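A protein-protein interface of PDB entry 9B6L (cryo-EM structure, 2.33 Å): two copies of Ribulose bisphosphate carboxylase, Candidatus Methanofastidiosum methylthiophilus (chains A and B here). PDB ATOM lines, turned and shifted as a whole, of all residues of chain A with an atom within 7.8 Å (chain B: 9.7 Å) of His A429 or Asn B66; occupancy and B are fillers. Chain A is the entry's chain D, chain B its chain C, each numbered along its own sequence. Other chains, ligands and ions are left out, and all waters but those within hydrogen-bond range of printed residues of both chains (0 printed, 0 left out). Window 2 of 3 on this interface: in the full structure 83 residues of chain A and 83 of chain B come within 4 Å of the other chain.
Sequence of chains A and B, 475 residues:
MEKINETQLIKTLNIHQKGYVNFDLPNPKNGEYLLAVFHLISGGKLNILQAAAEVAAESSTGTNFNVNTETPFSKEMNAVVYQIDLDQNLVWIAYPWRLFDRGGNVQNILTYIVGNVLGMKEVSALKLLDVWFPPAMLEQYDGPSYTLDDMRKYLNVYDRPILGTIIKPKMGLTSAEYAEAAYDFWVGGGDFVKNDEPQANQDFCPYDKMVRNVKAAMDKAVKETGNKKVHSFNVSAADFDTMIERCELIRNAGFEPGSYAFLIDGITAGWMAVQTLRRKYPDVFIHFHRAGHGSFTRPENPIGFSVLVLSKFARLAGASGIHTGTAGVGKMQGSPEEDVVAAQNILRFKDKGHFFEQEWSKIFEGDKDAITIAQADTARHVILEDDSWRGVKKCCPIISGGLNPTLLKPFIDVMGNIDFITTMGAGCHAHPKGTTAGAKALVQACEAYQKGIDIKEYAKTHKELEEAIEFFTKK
No position is printed for both chains.
Among the printed residues, pairs that only touch across the chains: Lys A168 with Val B67 (3.99 Å), Pro A169 with Thr B63 (3.3 Å), Pro A169 with Thr B69 (3.5 Å), Pro A169 with Glu B70 (3.9 Å), Ala A426 with Phe B65 (3.6 Å) and His A429 with Val B67 (3.5 Å).
Printed residues of chain B that touch a printed residue of chain A: Gly B62, Thr B63, Phe B65, Asn B66, Val B67, Thr B69 and Glu B70. Hydrophobic or aromatic side chains of chain B that line the printed part of chain A: Phe B65 and Val B67. Along chain A the printed residues that touch a printed residue of chain B span positions 168 to 429. Among the printed residues, no Asp or Glu carboxylate lies within 4 Å of a Lys or Arg side-chain nitrogen of the other chain.
The backbone carbonyl oxygen (O) of Ile A166 lies within hydrogen-bond range of a ring nitrogen (NE2) of His A429, at 2.7 Å. OH of Tyr B20 sits at hydrogen-bond distance from N of Thr B63 (2.9 Å). A ring nitrogen (NE2) of His B16 sits at hydrogen-bond distance from the backbone NH (N) of Asn B66, at 3.2 Å. The side-chain hydroxyl (OH) of Tyr B20 lies within hydrogen-bond range of the backbone NH (N) of Gly B62, at 3.5 Å. O of Gly A425 sits at hydrogen-bond distance from ND1 of His A429 (2.5 Å).
His A429 touches two residues of chain B. Asn B66 touches just one residue of chain A: His A429. No residue of chain B comes within 4 Å of Gly A425. Gly A427 touches none of the printed residues of chain B. No residue of chain B comes within 4 Å of Cys A428. Of the printed residues of chain A, Thr B69 touches Lys A168 and Pro A169. Of the printed residues of chain A, Glu B70 touches Pro A169. Asn B64 touches none of the printed residues of chain A.
O of His A429 lies close to O of Asn B66. The side-chain hydroxyl (OG1) of Thr B69 lies within hydrogen-bond range of the backbone carbonyl oxygen (O) of Lys A168 (2.4 Å). O of Gly B62 lies within hydrogen-bond range of NZ of Lys A168 (2.9 Å).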
ATOM      1  N   GLY A 164     -17.485  36.549  -7.510  1.00  0.00           N
ATOM      2  CA  GLY A 164     -18.910  36.313  -7.532  1.00  0.00           C
ATOM      3  C   GLY A 164     -19.243  35.011  -8.237  1.00  0.00           C
ATOM      4  O   GLY A 164     -18.416  34.426  -8.936  1.00  0.00           O
ATOM      5  N   THR A 165     -20.483  34.571  -8.038  1.00  0.00           N
ATOM      6  CA  THR A 165     -20.969  33.364  -8.687  1.00  0.00           C
ATOM      7  C   THR A 165     -22.464  33.481  -8.938  1.00  0.00           C
ATOM      8  O   THR A 165     -23.175  34.238  -8.271  1.00  0.00           O
ATOM      9  CB  THR A 165     -20.675  32.109  -7.852  1.00  0.00           C
ATOM     10  OG1 THR A 165     -20.630  30.960  -8.706  1.00  0.00           O
ATOM     11  CG2 THR A 165     -21.740  31.900  -6.784  1.00  0.00           C
ATOM     12  N   ILE A 166     -22.922  32.736  -9.936  1.00  0.00           N
ATOM     13  CA  ILE A 166     -24.331  32.421 -10.111  1.00  0.00           C
ATOM     14  C   ILE A 166     -24.542  31.003  -9.608  1.00  0.00           C
ATOM     15  O   ILE A 166     -23.634  30.166  -9.657  1.00  0.00           O
ATOM     16  CB  ILE A 166     -24.787  32.558 -11.579  1.00  0.00           C
ATOM     17  CG1 ILE A 166     -23.919  31.687 -12.488  1.00  0.00           C
ATOM     18  CG2 ILE A 166     -24.751  34.012 -12.016  1.00  0.00           C
ATOM     19  CD1 ILE A 166     -24.478  31.494 -13.875  1.00  0.00           C
ATOM     20  N   ILE A 167     -25.740  30.732  -9.115  1.00  0.00           N
ATOM     21  CA  ILE A 167     -26.076  29.410  -8.601  1.00  0.00           C
ATOM     22  C   ILE A 167     -26.631  28.565  -9.737  1.00  0.00           C
ATOM     23  O   ILE A 167     -27.578  28.967 -10.421  1.00  0.00           O
ATOM     24  CB  ILE A 167     -27.078  29.508  -7.441  1.00  0.00           C
ATOM     25  CG1 ILE A 167     -26.423  30.172  -6.226  1.00  0.00           C
ATOM     26  CG2 ILE A 167     -27.619  28.133  -7.088  1.00  0.00           C
ATOM     27  CD1 ILE A 167     -25.047  29.640  -5.893  1.00  0.00           C
ATOM     28  N   LYS A 168     -26.034  27.393  -9.943  1.00  0.00           N
ATOM     29  CA  LYS A 168     -26.494  26.424 -10.921  1.00  0.00           C
ATOM     30  C   LYS A 168     -27.138  25.247 -10.208  1.00  0.00           C
ATOM     31  O   LYS A 168     -26.526  24.685  -9.292  1.00  0.00           O
ATOM     32  CB  LYS A 168     -25.334  25.935 -11.791  1.00  0.00           C
ATOM     33  CG  LYS A 168     -24.725  27.007 -12.678  1.00  0.00           C
ATOM     34  CD  LYS A 168     -25.665  27.386 -13.807  1.00  0.00           C
ATOM     35  CE  LYS A 168     -24.899  27.729 -15.073  1.00  0.00           C
ATOM     36  NZ  LYS A 168     -25.792  28.271 -16.131  1.00  0.00           N
ATOM     37  N   PRO A 169     -28.359  24.835 -10.585  1.00  0.00           N
ATOM     38  CA  PRO A 169     -29.211  25.354 -11.672  1.00  0.00           C
ATOM     39  C   PRO A 169     -29.691  26.783 -11.442  1.00  0.00           C
ATOM     40  O   PRO A 169     -29.822  27.225 -10.305  1.00  0.00           O
ATOM     41  CB  PRO A 169     -30.395  24.370 -11.684  1.00  0.00           C
ATOM     42  CG  PRO A 169     -29.881  23.125 -11.030  1.00  0.00           C
ATOM     43  CD  PRO A 169     -28.933  23.620  -9.983  1.00  0.00           C
ATOM     44  N   ALA A 181     -26.308  26.389  -1.694  1.00  0.00           N
ATOM     45  CA  ALA A 181     -25.312  26.618  -2.742  1.00  0.00           C
ATOM     46  C   ALA A 181     -24.595  27.952  -2.544  1.00  0.00           C
ATOM     47  O   ALA A 181     -23.373  28.050  -2.738  1.00  0.00           O
ATOM     48  CB  ALA A 181     -25.975  26.556  -4.116  1.00  0.00           C
ATOM     49  N   PHE A 185     -20.517  28.443  -1.901  1.00  0.00           N
ATOM     50  CA  PHE A 185     -19.599  29.360  -2.573  1.00  0.00           C
ATOM     51  C   PHE A 185     -18.958  30.332  -1.588  1.00  0.00           C
ATOM     52  O   PHE A 185     -17.749  30.580  -1.651  1.00  0.00           O
ATOM     53  CB  PHE A 185     -20.313  30.124  -3.685  1.00  0.00           C
ATOM     54  CG  PHE A 185     -19.429  31.104  -4.400  1.00  0.00           C
ATOM     55  CD1 PHE A 185     -18.536  30.674  -5.366  1.00  0.00           C
ATOM     56  CD2 PHE A 185     -19.494  32.456  -4.111  1.00  0.00           C
ATOM     57  CE1 PHE A 185     -17.723  31.572  -6.024  1.00  0.00           C
ATOM     58  CE2 PHE A 185     -18.690  33.355  -4.771  1.00  0.00           C
ATOM     59  CZ  PHE A 185     -17.803  32.914  -5.727  1.00  0.00           C
ATOM     60  N   GLY A 402     -17.791  31.537 -16.909  1.00  0.00           N
ATOM     61  CA  GLY A 402     -16.660  30.635 -17.021  1.00  0.00           C
ATOM     62  C   GLY A 402     -15.282  31.186 -16.718  1.00  0.00           C
ATOM     63  O   GLY A 402     -14.350  30.967 -17.497  1.00  0.00           O
ATOM     64  N   THR A 423     -18.757  37.298 -11.694  1.00  0.00           N
ATOM     65  CA  THR A 423     -19.677  36.218 -11.340  1.00  0.00           C
ATOM     66  C   THR A 423     -19.434  35.049 -12.284  1.00  0.00           C
ATOM     67  O   THR A 423     -19.844  35.078 -13.445  1.00  0.00           O
ATOM     68  CB  THR A 423     -21.125  36.692 -11.406  1.00  0.00           C
ATOM     69  OG1 THR A 423     -21.448  37.061 -12.752  1.00  0.00           O
ATOM     70  CG2 THR A 423     -21.340  37.889 -10.493  1.00  0.00           C
ATOM     71  N   MET A 424     -18.776  34.008 -11.782  1.00  0.00           N
ATOM     72  CA  MET A 424     -18.443  32.863 -12.619  1.00  0.00           C
ATOM     73  C   MET A 424     -19.693  32.071 -12.980  1.00  0.00           C
ATOM     74  O   MET A 424     -20.605  31.907 -12.167  1.00  0.00           O
ATOM     75  CB  MET A 424     -17.436  31.958 -11.909  1.00  0.00           C
ATOM     76  CG  MET A 424     -17.744  31.705 -10.443  1.00  0.00           C
ATOM     77  SD  MET A 424     -16.636  30.489  -9.707  1.00  0.00           S
ATOM     78  CE  MET A 424     -17.738  29.091  -9.521  1.00  0.00           C
ATOM     79  N   GLY A 425     -19.728  31.584 -14.218  1.00  0.00           N
ATOM     80  CA  GLY A 425     -20.806  30.736 -14.682  1.00  0.00           C
ATOM     81  C   GLY A 425     -20.402  29.277 -14.728  1.00  0.00           C
ATOM     82  O   GLY A 425     -20.380  28.599 -13.697  1.00  0.00           O
ATOM     83  N   ALA A 426     -20.075  28.784 -15.922  1.00  0.00           N
ATOM     84  CA  ALA A 426     -19.668  27.400 -16.129  1.00  0.00           C
ATOM     85  C   ALA A 426     -18.211  27.138 -15.752  1.00  0.00           C
ATOM     86  O   ALA A 426     -17.678  26.084 -16.118  1.00  0.00           O
ATOM     87  CB  ALA A 426     -19.906  26.998 -17.587  1.00  0.00           C
ATOM     88  N   GLY A 427     -17.563  28.062 -15.040  1.00  0.00           N
ATOM     89  CA  GLY A 427     -16.135  27.923 -14.789  1.00  0.00           C
ATOM     90  C   GLY A 427     -15.788  26.703 -13.959  1.00  0.00           C
ATOM     91  O   GLY A 427     -14.868  25.952 -14.292  1.00  0.00           O
ATOM     92  N   CYS A 428     -16.519  26.486 -12.863  1.00  0.00           N
ATOM     93  CA  CYS A 428     -16.190  25.393 -11.957  1.00  0.00           C
ATOM     94  C   CYS A 428     -17.415  24.655 -11.431  1.00  0.00           C
ATOM     95  O   CYS A 428     -17.264  23.771 -10.577  1.00  0.00           O
ATOM     96  CB  CYS A 428     -15.357  25.910 -10.776  1.00  0.00           C
ATOM     97  SG  CYS A 428     -13.725  26.541 -11.230  1.00  0.00           S
ATOM     98  N   HIS A 429     -18.613  24.982 -11.901  1.00  0.00           N
ATOM     99  CA  HIS A 429     -19.824  24.342 -11.402  1.00  0.00           C
ATOM    100  C   HIS A 429     -19.886  22.876 -11.819  1.00  0.00           C
ATOM    101  O   HIS A 429     -20.257  22.010 -11.026  1.00  0.00           O
ATOM    102  CB  HIS A 429     -21.064  25.084 -11.902  1.00  0.00           C
ATOM    103  CG  HIS A 429     -21.372  26.332 -11.136  1.00  0.00           C
ATOM    104  ND1 HIS A 429     -20.812  27.552 -11.448  1.00  0.00           N
ATOM    105  CD2 HIS A 429     -22.185  26.551 -10.076  1.00  0.00           C
ATOM    106  CE1 HIS A 429     -21.264  28.468 -10.611  1.00  0.00           C
ATOM    107  NE2 HIS A 429     -22.100  27.887  -9.769  1.00  0.00           N
ATOM    108  N   PRO A 432     -15.780  17.929  -9.458  1.00  0.00           N
ATOM    109  CA  PRO A 432     -16.160  16.908  -8.477  1.00  0.00           C
ATOM    110  C   PRO A 432     -15.540  17.153  -7.104  1.00  0.00           C
ATOM    111  O   PRO A 432     -15.863  16.445  -6.150  1.00  0.00           O
ATOM    112  CB  PRO A 432     -15.625  15.614  -9.094  1.00  0.00           C
ATOM    113  CG  PRO A 432     -14.473  16.050  -9.927  1.00  0.00           C
ATOM    114  CD  PRO A 432     -14.818  17.416 -10.449  1.00  0.00           C
ATOM    115  N   GLY A 434     -15.992  19.897  -5.409  1.00  0.00           N
ATOM    116  CA  GLY A 434     -16.894  20.728  -4.643  1.00  0.00           C
ATOM    117  C   GLY A 434     -16.798  22.192  -5.037  1.00  0.00           C
ATOM    118  O   GLY A 434     -15.753  22.680  -5.490  1.00  0.00           O
ATOM    119  N   THR A 435     -17.914  22.905  -4.867  1.00  0.00           N
ATOM    120  CA  THR A 435     -17.933  24.340  -5.133  1.00  0.00           C
ATOM    121  C   THR A 435     -17.007  25.087  -4.182  1.00  0.00           C
ATOM    122  O   THR A 435     -16.358  26.065  -4.575  1.00  0.00           O
ATOM    123  CB  THR A 435     -19.365  24.871  -5.020  1.00  0.00           C
ATOM    124  OG1 THR A 435     -20.199  24.203  -5.975  1.00  0.00           O
ATOM    125  CG2 THR A 435     -19.410  26.369  -5.284  1.00  0.00           C
ATOM    126  N   GLY A 438     -13.498  24.944  -5.490  1.00  0.00           N
ATOM    127  CA  GLY A 438     -13.310  25.857  -6.607  1.00  0.00           C
ATOM    128  C   GLY A 438     -13.210  27.307  -6.171  1.00  0.00           C
ATOM    129  O   GLY A 438     -12.390  28.069  -6.690  1.00  0.00           O
ATOM    130  N   ASN B  14     -25.554  16.397 -25.907  1.00  0.00           N
ATOM    131  CA  ASN B  14     -25.081  15.795 -24.672  1.00  0.00           C
ATOM    132  C   ASN B  14     -26.268  15.588 -23.730  1.00  0.00           C
ATOM    133  O   ASN B  14     -27.395  16.005 -24.011  1.00  0.00           O
ATOM    134  CB  ASN B  14     -23.986  16.655 -24.041  1.00  0.00           C
ATOM    135  CG  ASN B  14     -24.470  18.039 -23.660  1.00  0.00           C
ATOM    136  OD1 ASN B  14     -25.090  18.228 -22.615  1.00  0.00           O
ATOM    137  ND2 ASN B  14     -24.173  19.020 -24.502  1.00  0.00           N
ATOM    138  N   ILE B  15     -26.019  14.925 -22.598  1.00  0.00           N
ATOM    139  CA  ILE B  15     -27.110  14.576 -21.693  1.00  0.00           C
ATOM    140  C   ILE B  15     -27.782  15.829 -21.138  1.00  0.00           C
ATOM    141  O   ILE B  15     -29.014  15.893 -21.029  1.00  0.00           O
ATOM    142  CB  ILE B  15     -26.604  13.645 -20.573  1.00  0.00           C
ATOM    143  CG1 ILE B  15     -25.448  14.287 -19.802  1.00  0.00           C
ATOM    144  CG2 ILE B  15     -26.184  12.302 -21.148  1.00  0.00           C
ATOM    145  CD1 ILE B  15     -25.640  14.274 -18.303  1.00  0.00           C
ATOM    146  N   HIS B  16     -26.990  16.845 -20.787  1.00  0.00           N
ATOM    147  CA  HIS B  16     -27.566  18.087 -20.283  1.00  0.00           C
ATOM    148  C   HIS B  16     -28.410  18.773 -21.350  1.00  0.00           C
ATOM    149  O   HIS B  16     -29.482  19.311 -21.052  1.00  0.00           O
ATOM    150  CB  HIS B  16     -26.456  19.014 -19.790  1.00  0.00           C
ATOM    151  CG  HIS B  16     -25.346  18.301 -19.086  1.00  0.00           C
ATOM    152  ND1 HIS B  16     -24.107  18.105 -19.655  1.00  0.00           N
ATOM    153  CD2 HIS B  16     -25.289  17.733 -17.858  1.00  0.00           C
ATOM    154  CE1 HIS B  16     -23.334  17.449 -18.809  1.00  0.00           C
ATOM    155  NE2 HIS B  16     -24.027  17.210 -17.710  1.00  0.00           N
ATOM    156  N   GLN B  17     -27.943  18.762 -22.599  1.00  0.00           N
ATOM    157  CA  GLN B  17     -28.747  19.292 -23.695  1.00  0.00           C
ATOM    158  C   GLN B  17     -29.968  18.421 -23.953  1.00  0.00           C
ATOM    159  O   GLN B  17     -31.045  18.933 -24.280  1.00  0.00           O
ATOM    160  CB  GLN B  17     -27.900  19.412 -24.959  1.00  0.00           C
ATOM    161  CG  GLN B  17     -27.096  20.689 -25.039  1.00  0.00           C
ATOM    162  CD  GLN B  17     -26.187  20.730 -26.247  1.00  0.00           C
ATOM    163  OE1 GLN B  17     -26.116  19.775 -27.017  1.00  0.00           O
ATOM    164  NE2 GLN B  17     -25.486  21.842 -26.421  1.00  0.00           N
ATOM    165  N   TYR B  20     -33.229  19.225 -22.182  1.00  0.00           N
ATOM    166  CA  TYR B  20     -34.036  20.363 -22.607  1.00  0.00           C
ATOM    167  C   TYR B  20     -34.726  20.135 -23.943  1.00  0.00           C
ATOM    168  O   TYR B  20     -35.315  21.071 -24.492  1.00  0.00           O
ATOM    169  CB  TYR B  20     -33.173  21.625 -22.664  1.00  0.00           C
ATOM    170  CG  TYR B  20     -32.740  22.097 -21.301  1.00  0.00           C
ATOM    171  CD1 TYR B  20     -33.588  22.855 -20.508  1.00  0.00           C
ATOM    172  CD2 TYR B  20     -31.499  21.751 -20.790  1.00  0.00           C
ATOM    173  CE1 TYR B  20     -33.200  23.278 -19.256  1.00  0.00           C
ATOM    174  CE2 TYR B  20     -31.105  22.166 -19.538  1.00  0.00           C
ATOM    175  CZ  TYR B  20     -31.958  22.926 -18.774  1.00  0.00           C
ATOM    176  OH  TYR B  20     -31.565  23.342 -17.527  1.00  0.00           O
ATOM    177  N   GLY B  62     -30.868  26.721 -17.026  1.00  0.00           N
ATOM    178  CA  GLY B  62     -29.435  26.867 -17.226  1.00  0.00           C
ATOM    179  C   GLY B  62     -28.591  25.731 -16.695  1.00  0.00           C
ATOM    180  O   GLY B  62     -27.550  25.977 -16.074  1.00  0.00           O
ATOM    181  N   THR B  63     -29.012  24.492 -16.920  1.00  0.00           N
ATOM    182  CA  THR B  63     -28.215  23.331 -16.542  1.00  0.00           C
ATOM    183  C   THR B  63     -27.733  22.667 -17.829  1.00  0.00           C
ATOM    184  O   THR B  63     -28.307  21.689 -18.307  1.00  0.00           O
ATOM    185  CB  THR B  63     -29.020  22.366 -15.669  1.00  0.00           C
ATOM    186  OG1 THR B  63     -29.756  23.107 -14.690  1.00  0.00           O
ATOM    187  CG2 THR B  63     -28.091  21.401 -14.958  1.00  0.00           C
ATOM    188  N   ASN B  64     -26.645  23.202 -18.375  1.00  0.00           N
ATOM    189  CA  ASN B  64     -26.010  22.657 -19.566  1.00  0.00           C
ATOM    190  C   ASN B  64     -24.700  21.956 -19.241  1.00  0.00           C
ATOM    191  O   ASN B  64     -23.999  21.509 -20.154  1.00  0.00           O
ATOM    192  CB  ASN B  64     -25.785  23.763 -20.599  1.00  0.00           C
ATOM    193  CG  ASN B  64     -25.219  25.026 -19.985  1.00  0.00           C
ATOM    194  OD1 ASN B  64     -25.309  25.238 -18.777  1.00  0.00           O
ATOM    195  ND2 ASN B  64     -24.631  25.876 -20.818  1.00  0.00           N
ATOM    196  N   PHE B  65     -24.357  21.852 -17.960  1.00  0.00           N
ATOM    197  CA  PHE B  65     -23.161  21.162 -17.506  1.00  0.00           C
ATOM    198  C   PHE B  65     -23.536  20.294 -16.314  1.00  0.00           C
ATOM    199  O   PHE B  65     -24.629  20.413 -15.753  1.00  0.00           O
ATOM    200  CB  PHE B  65     -22.049  22.149 -17.129  1.00  0.00           C
ATOM    201  CG  PHE B  65     -21.521  22.942 -18.289  1.00  0.00           C
ATOM    202  CD1 PHE B  65     -22.164  24.096 -18.706  1.00  0.00           C
ATOM    203  CD2 PHE B  65     -20.380  22.538 -18.960  1.00  0.00           C
ATOM    204  CE1 PHE B  65     -21.681  24.828 -19.772  1.00  0.00           C
ATOM    205  CE2 PHE B  65     -19.892  23.267 -20.027  1.00  0.00           C
ATOM    206  CZ  PHE B  65     -20.543  24.415 -20.433  1.00  0.00           C
ATOM    207  N   ASN B  66     -22.619  19.416 -15.925  1.00  0.00           N
ATOM    208  CA  ASN B  66     -22.855  18.519 -14.798  1.00  0.00           C
ATOM    209  C   ASN B  66     -22.626  19.282 -13.499  1.00  0.00           C
ATOM    210  O   ASN B  66     -21.509  19.731 -13.222  1.00  0.00           O
ATOM    211  CB  ASN B  66     -21.946  17.298 -14.884  1.00  0.00           C
ATOM    212  CG  ASN B  66     -22.044  16.414 -13.657  1.00  0.00           C
ATOM    213  OD1 ASN B  66     -23.030  15.701 -13.469  1.00  0.00           O
ATOM    214  ND2 ASN B  66     -21.024  16.463 -12.809  1.00  0.00           N
ATOM    215  N   VAL B  67     -23.683  19.437 -12.705  1.00  0.00           N
ATOM    216  CA  VAL B  67     -23.599  20.059 -11.391  1.00  0.00           C
ATOM    217  C   VAL B  67     -24.244  19.127 -10.376  1.00  0.00           C
ATOM    218  O   VAL B  67     -25.290  18.524 -10.647  1.00  0.00           O
ATOM    219  CB  VAL B  67     -24.267  21.453 -11.364  1.00  0.00           C
ATOM    220  CG1 VAL B  67     -23.486  22.428 -12.227  1.00  0.00           C
ATOM    221  CG2 VAL B  67     -25.714  21.377 -11.827  1.00  0.00           C
ATOM    222  N   ASN B  68     -23.609  18.989  -9.213  1.00  0.00           N
ATOM    223  CA  ASN B  68     -24.164  18.155  -8.155  1.00  0.00           C
ATOM    224  C   ASN B  68     -25.371  18.788  -7.478  1.00  0.00           C
ATOM    225  O   ASN B  68     -26.045  18.113  -6.694  1.00  0.00           O
ATOM    226  CB  ASN B  68     -23.092  17.840  -7.109  1.00  0.00           C
ATOM    227  CG  ASN B  68     -22.458  19.085  -6.527  1.00  0.00           C
ATOM    228  OD1 ASN B  68     -22.431  20.138  -7.164  1.00  0.00           O
ATOM    229  ND2 ASN B  68     -21.944  18.972  -5.308  1.00  0.00           N
ATOM    230  N   THR B  69     -25.657  20.057  -7.761  1.00  0.00           N
ATOM    231  CA  THR B  69     -26.812  20.744  -7.203  1.00  0.00           C
ATOM    232  C   THR B  69     -28.077  20.531  -8.021  1.00  0.00           C
ATOM    233  O   THR B  69     -29.133  21.051  -7.645  1.00  0.00           O
ATOM    234  CB  THR B  69     -26.528  22.246  -7.086  1.00  0.00           C
ATOM    235  OG1 THR B  69     -25.728  22.669  -8.195  1.00  0.00           O
ATOM    236  CG2 THR B  69     -25.790  22.548  -5.794  1.00  0.00           C
ATOM    237  N   GLU B  70     -27.997  19.793  -9.126  1.00  0.00           N
ATOM    238  CA  GLU B  70     -29.180  19.502  -9.922  1.00  0.00           C
ATOM    239  C   GLU B  70     -30.140  18.612  -9.143  1.00  0.00           C
ATOM    240  O   GLU B  70     -29.734  17.634  -8.511  1.00  0.00           O
ATOM    241  CB  GLU B  70     -28.781  18.826 -11.234  1.00  0.00           C
ATOM    242  CG  GLU B  70     -29.757  19.055 -12.379  1.00  0.00           C
ATOM    243  CD  GLU B  70     -29.591  18.041 -13.494  1.00  0.00           C
ATOM    244  OE1 GLU B  70     -29.907  16.854 -13.271  1.00  0.00           O
ATOM    245  OE2 GLU B  70     -29.149  18.427 -14.596  1.00  0.00           O
